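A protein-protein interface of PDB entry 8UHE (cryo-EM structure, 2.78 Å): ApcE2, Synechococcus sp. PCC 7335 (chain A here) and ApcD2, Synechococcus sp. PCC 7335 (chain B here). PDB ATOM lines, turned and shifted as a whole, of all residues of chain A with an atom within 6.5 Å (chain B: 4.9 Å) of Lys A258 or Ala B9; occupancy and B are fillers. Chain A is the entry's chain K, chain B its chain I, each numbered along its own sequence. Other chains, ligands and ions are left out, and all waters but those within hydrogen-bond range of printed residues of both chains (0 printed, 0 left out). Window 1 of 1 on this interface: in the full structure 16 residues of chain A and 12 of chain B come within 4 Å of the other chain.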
ATOM      1  N   GLY A 255     -19.291 -12.668 -18.298  1.00  0.00           N
ATOM      2  CA  GLY A 255     -19.792 -11.566 -17.506  1.00  0.00           C
ATOM      3  C   GLY A 255     -20.189 -11.959 -16.103  1.00  0.00           C
ATOM      4  O   GLY A 255     -20.940 -12.919 -15.917  1.00  0.00           O
ATOM      5  N   VAL A 256     -19.691 -11.225 -15.103  1.00  0.00           N
ATOM      6  CA  VAL A 256     -19.918 -11.599 -13.710  1.00  0.00           C
ATOM      7  C   VAL A 256     -21.215 -11.023 -13.153  1.00  0.00           C
ATOM      8  O   VAL A 256     -21.661 -11.454 -12.079  1.00  0.00           O
ATOM      9  CB  VAL A 256     -18.717 -11.170 -12.844  1.00  0.00           C
ATOM     10  CG1 VAL A 256     -17.510 -12.076 -13.115  1.00  0.00           C
ATOM     11  CG2 VAL A 256     -18.364  -9.712 -13.085  1.00  0.00           C
ATOM     12  N   SER A 257     -21.840 -10.080 -13.853  1.00  0.00           N
ATOM     13  CA  SER A 257     -23.093  -9.479 -13.415  1.00  0.00           C
ATOM     14  C   SER A 257     -23.794  -8.918 -14.643  1.00  0.00           C
ATOM     15  O   SER A 257     -23.237  -8.905 -15.743  1.00  0.00           O
ATOM     16  CB  SER A 257     -22.854  -8.389 -12.365  1.00  0.00           C
ATOM     17  OG  SER A 257     -23.912  -8.343 -11.423  1.00  0.00           O
ATOM     18  N   LYS A 258     -25.029  -8.445 -14.435  1.00  0.00           N
ATOM     19  CA  LYS A 258     -25.812  -7.857 -15.522  1.00  0.00           C
ATOM     20  C   LYS A 258     -25.131  -6.632 -16.117  1.00  0.00           C
ATOM     21  O   LYS A 258     -25.328  -6.320 -17.297  1.00  0.00           O
ATOM     22  CB  LYS A 258     -27.203  -7.480 -15.017  1.00  0.00           C
ATOM     23  CG  LYS A 258     -27.556  -8.114 -13.688  1.00  0.00           C
ATOM     24  CD  LYS A 258     -28.945  -7.727 -13.225  1.00  0.00           C
ATOM     25  CE  LYS A 258     -29.017  -6.267 -12.818  1.00  0.00           C
ATOM     26  NZ  LYS A 258     -30.385  -5.914 -12.352  1.00  0.00           N
ATOM     27  N   HIS A 259     -24.338  -5.927 -15.321  1.00  0.00           N
ATOM     28  CA  HIS A 259     -23.606  -4.772 -15.805  1.00  0.00           C
ATOM     29  C   HIS A 259     -22.261  -5.130 -16.422  1.00  0.00           C
ATOM     30  O   HIS A 259     -21.652  -4.281 -17.080  1.00  0.00           O
ATOM     31  CB  HIS A 259     -23.410  -3.782 -14.658  1.00  0.00           C
ATOM     32  CG  HIS A 259     -24.613  -3.628 -13.778  1.00  0.00           C
ATOM     33  ND1 HIS A 259     -25.710  -2.878 -14.141  1.00  0.00           N
ATOM     34  CD2 HIS A 259     -24.887  -4.124 -12.548  1.00  0.00           C
ATOM     35  CE1 HIS A 259     -26.607  -2.913 -13.172  1.00  0.00           C
ATOM     36  NE2 HIS A 259     -26.133  -3.664 -12.194  1.00  0.00           N
ATOM     37  N   ASP A 260     -21.795  -6.364 -16.252  1.00  0.00           N
ATOM     38  CA  ASP A 260     -20.492  -6.783 -16.749  1.00  0.00           C
ATOM     39  C   ASP A 260     -20.676  -7.508 -18.076  1.00  0.00           C
ATOM     40  O   ASP A 260     -21.369  -8.530 -18.139  1.00  0.00           O
ATOM     41  CB  ASP A 260     -19.787  -7.675 -15.727  1.00  0.00           C
ATOM     42  CG  ASP A 260     -18.398  -8.104 -16.174  1.00  0.00           C
ATOM     43  OD1 ASP A 260     -18.280  -8.909 -17.104  1.00  0.00           O
ATOM     44  OD2 ASP A 260     -17.402  -7.628 -15.594  1.00  0.00           O
ATOM     45  N   GLN A 261     -20.035  -6.999 -19.122  1.00  0.00           N
ATOM     46  CA  GLN A 261     -20.100  -7.651 -20.419  1.00  0.00           C
ATOM     47  C   GLN A 261     -19.181  -8.864 -20.440  1.00  0.00           C
ATOM     48  O   GLN A 261     -18.098  -8.856 -19.853  1.00  0.00           O
ATOM     49  CB  GLN A 261     -19.725  -6.679 -21.540  1.00  0.00           C
ATOM     50  CG  GLN A 261     -18.314  -6.126 -21.492  1.00  0.00           C
ATOM     51  CD  GLN A 261     -17.904  -5.467 -22.793  1.00  0.00           C
ATOM     52  OE1 GLN A 261     -18.518  -5.689 -23.836  1.00  0.00           O
ATOM     53  NE2 GLN A 261     -16.866  -4.647 -22.736  1.00  0.00           N
ATOM     54  N   GLY A 262     -19.633  -9.924 -21.095  1.00  0.00           N
ATOM     55  CA  GLY A 262     -18.776 -11.066 -21.300  1.00  0.00           C
ATOM     56  C   GLY A 262     -17.874 -10.872 -22.502  1.00  0.00           C
ATOM     57  O   GLY A 262     -18.250 -10.269 -23.505  1.00  0.00           O
ATOM     58  N   GLU A 371     -21.654   0.385 -11.814  1.00  0.00           N
ATOM     59  CA  GLU A 371     -22.540  -0.237 -10.828  1.00  0.00           C
ATOM     60  C   GLU A 371     -21.770  -1.116  -9.845  1.00  0.00           C
ATOM     61  O   GLU A 371     -22.140  -1.215  -8.665  1.00  0.00           O
ATOM     62  CB  GLU A 371     -23.620  -1.038 -11.552  1.00  0.00           C
ATOM     63  CG  GLU A 371     -24.346  -0.247 -12.638  1.00  0.00           C
ATOM     64  CD  GLU A 371     -23.727  -0.414 -14.018  1.00  0.00           C
ATOM     65  OE1 GLU A 371     -22.491  -0.310 -14.134  1.00  0.00           O
ATOM     66  OE2 GLU A 371     -24.474  -0.656 -14.989  1.00  0.00           O
ATOM     67  N   SER B   5     -33.927  -6.135 -21.878  1.00  0.00           N
ATOM     68  CA  SER B   5     -32.624  -5.682 -21.405  1.00  0.00           C
ATOM     69  C   SER B   5     -31.906  -6.769 -20.617  1.00  0.00           C
ATOM     70  O   SER B   5     -30.708  -7.000 -20.813  1.00  0.00           O
ATOM     71  CB  SER B   5     -32.795  -4.437 -20.538  1.00  0.00           C
ATOM     72  OG  SER B   5     -33.312  -4.784 -19.263  1.00  0.00           O
ATOM     73  N   GLN B   6     -32.626  -7.461 -19.733  1.00  0.00           N
ATOM     74  CA  GLN B   6     -31.975  -8.485 -18.928  1.00  0.00           C
ATOM     75  C   GLN B   6     -31.680  -9.736 -19.737  1.00  0.00           C
ATOM     76  O   GLN B   6     -30.708 -10.434 -19.445  1.00  0.00           O
ATOM     77  CB  GLN B   6     -32.830  -8.839 -17.721  1.00  0.00           C
ATOM     78  CG  GLN B   6     -34.240  -9.151 -18.082  1.00  0.00           C
ATOM     79  CD  GLN B   6     -35.020  -9.668 -16.920  1.00  0.00           C
ATOM     80  OE1 GLN B   6     -34.564  -9.616 -15.778  1.00  0.00           O
ATOM     81  NE2 GLN B   6     -36.205 -10.185 -17.195  1.00  0.00           N
ATOM     82  N   VAL B   7     -32.492 -10.043 -20.751  1.00  0.00           N
ATOM     83  CA  VAL B   7     -32.169 -11.199 -21.576  1.00  0.00           C
ATOM     84  C   VAL B   7     -30.967 -10.888 -22.469  1.00  0.00           C
ATOM     85  O   VAL B   7     -30.125 -11.762 -22.730  1.00  0.00           O
ATOM     86  CB  VAL B   7     -33.423 -11.662 -22.347  1.00  0.00           C
ATOM     87  CG1 VAL B   7     -33.691 -10.867 -23.629  1.00  0.00           C
ATOM     88  CG2 VAL B   7     -33.358 -13.136 -22.586  1.00  0.00           C
ATOM     89  N   ILE B   8     -30.818  -9.618 -22.868  1.00  0.00           N
ATOM     90  CA  ILE B   8     -29.607  -9.161 -23.541  1.00  0.00           C
ATOM     91  C   ILE B   8     -28.404  -9.289 -22.616  1.00  0.00           C
ATOM     92  O   ILE B   8     -27.342  -9.775 -23.020  1.00  0.00           O
ATOM     93  CB  ILE B   8     -29.803  -7.715 -24.036  1.00  0.00           C
ATOM     94  CG1 ILE B   8     -30.573  -7.704 -25.356  1.00  0.00           C
ATOM     95  CG2 ILE B   8     -28.476  -6.976 -24.174  1.00  0.00           C
ATOM     96  CD1 ILE B   8     -31.053  -6.335 -25.761  1.00  0.00           C
ATOM     97  N   ALA B   9     -28.560  -8.873 -21.355  1.00  0.00           N
ATOM     98  CA  ALA B   9     -27.463  -8.951 -20.392  1.00  0.00           C
ATOM     99  C   ALA B   9     -27.077 -10.398 -20.098  1.00  0.00           C
ATOM    100  O   ALA B   9     -25.891 -10.709 -19.931  1.00  0.00           O
ATOM    101  CB  ALA B   9     -27.847  -8.225 -19.104  1.00  0.00           C
ATOM    102  N   THR B  10     -28.065 -11.293 -20.029  1.00  0.00           N
ATOM    103  CA  THR B  10     -27.798 -12.708 -19.792  1.00  0.00           C
ATOM    104  C   THR B  10     -27.069 -13.345 -20.969  1.00  0.00           C
ATOM    105  O   THR B  10     -26.140 -14.138 -20.774  1.00  0.00           O
ATOM    106  CB  THR B  10     -29.111 -13.442 -19.511  1.00  0.00           C
ATOM    107  OG1 THR B  10     -29.741 -12.867 -18.360  1.00  0.00           O
ATOM    108  CG2 THR B  10     -28.867 -14.925 -19.260  1.00  0.00           C
ATOM    109  N   ALA B  11     -27.476 -13.012 -22.200  1.00  0.00           N
ATOM    110  CA  ALA B  11     -26.737 -13.493 -23.364  1.00  0.00           C
ATOM    111  C   ALA B  11     -25.333 -12.899 -23.408  1.00  0.00           C
ATOM    112  O   ALA B  11     -24.389 -13.552 -23.867  1.00  0.00           O
ATOM    113  CB  ALA B  11     -27.498 -13.169 -24.647  1.00  0.00           C
ATOM    114  N   ASP B  12     -25.181 -11.660 -22.938  1.00  0.00           N
ATOM    115  CA  ASP B  12     -23.863 -11.039 -22.897  1.00  0.00           C
ATOM    116  C   ASP B  12     -22.953 -11.733 -21.894  1.00  0.00           C
ATOM    117  O   ASP B  12     -21.756 -11.898 -22.146  1.00  0.00           O
ATOM    118  CB  ASP B  12     -23.995  -9.556 -22.559  1.00  0.00           C
ATOM    119  CG  ASP B  12     -22.803  -8.751 -23.017  1.00  0.00           C
ATOM    120  OD1 ASP B  12     -21.933  -9.310 -23.716  1.00  0.00           O
ATOM    121  OD2 ASP B  12     -22.735  -7.553 -22.685  1.00  0.00           O
ATOM    122  N   ARG B  13     -23.503 -12.143 -20.752  1.00  0.00           N
ATOM    123  CA  ARG B  13     -22.690 -12.742 -19.698  1.00  0.00           C
ATOM    124  C   ARG B  13     -22.155 -14.105 -20.112  1.00  0.00           C
ATOM    125  O   ARG B  13     -20.947 -14.356 -20.052  1.00  0.00           O
ATOM    126  CB  ARG B  13     -23.514 -12.866 -18.427  1.00  0.00           C
ATOM    127  CG  ARG B  13     -23.706 -11.571 -17.696  1.00  0.00           C
ATOM    128  CD  ARG B  13     -24.391 -11.865 -16.395  1.00  0.00           C
ATOM    129  NE  ARG B  13     -23.660 -12.899 -15.677  1.00  0.00           N
ATOM    130  CZ  ARG B  13     -23.834 -13.189 -14.397  1.00  0.00           C
ATOM    131  NH1 ARG B  13     -24.701 -12.526 -13.650  1.00  0.00           N
ATOM    132  NH2 ARG B  13     -23.120 -14.168 -13.852  1.00  0.00           N
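The guanidinium group (NE) of Arg B13 is in hydrogen-bond range of the backbone carbonyl oxygen (O) of Gly A255, 2.7 Å away.
The backbone carbonyl oxygen of Asp B12 is in hydrogen-bond range of the backbone NH of Gly A262 (3.1 Å).
The side-chain carboxylate (OD1) of Asp A260 lies within hydrogen-bond range of the backbone NH (N) of Val A256, 3.4 Å away.
Among the printed residues, pairs that only touch across the chains: Val A256 with Arg B13 (3.6 Å), Ser A257 with Arg B13 (3.2 Å), Lys A258 with Ala B9 (3.6 Å), Lys A258 with Arg B13 (3.99 Å), Asp A260 with Arg B13 (3.9 Å) and Gln A261 with Asp B12 (3.3 Å).
Of the printed residues of chain B, Gly A255 touches Arg B13 (2.7 Å).
Of the printed residues of chain B, Val A256 touches Arg B13.
Printed residues of chain B within 4 Å of Ser A257: Arg B13.
Printed residues of chain B within 4 Å of Gly A262: Asp B12.
Of chain A, only Lys A258 (3.6 Å) comes within 4 Å of Ala B9.
The nearest printed residue of chain B that does not touch Lys A258 is Gln B6 (6.0 Å).
The nearest printed residue of chain B that does not touch Gly A255 is Asp B12 (4.6 Å).
Hydrophobic or aromatic side chains of chain B that line the printed part of chain A: Ala B9.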
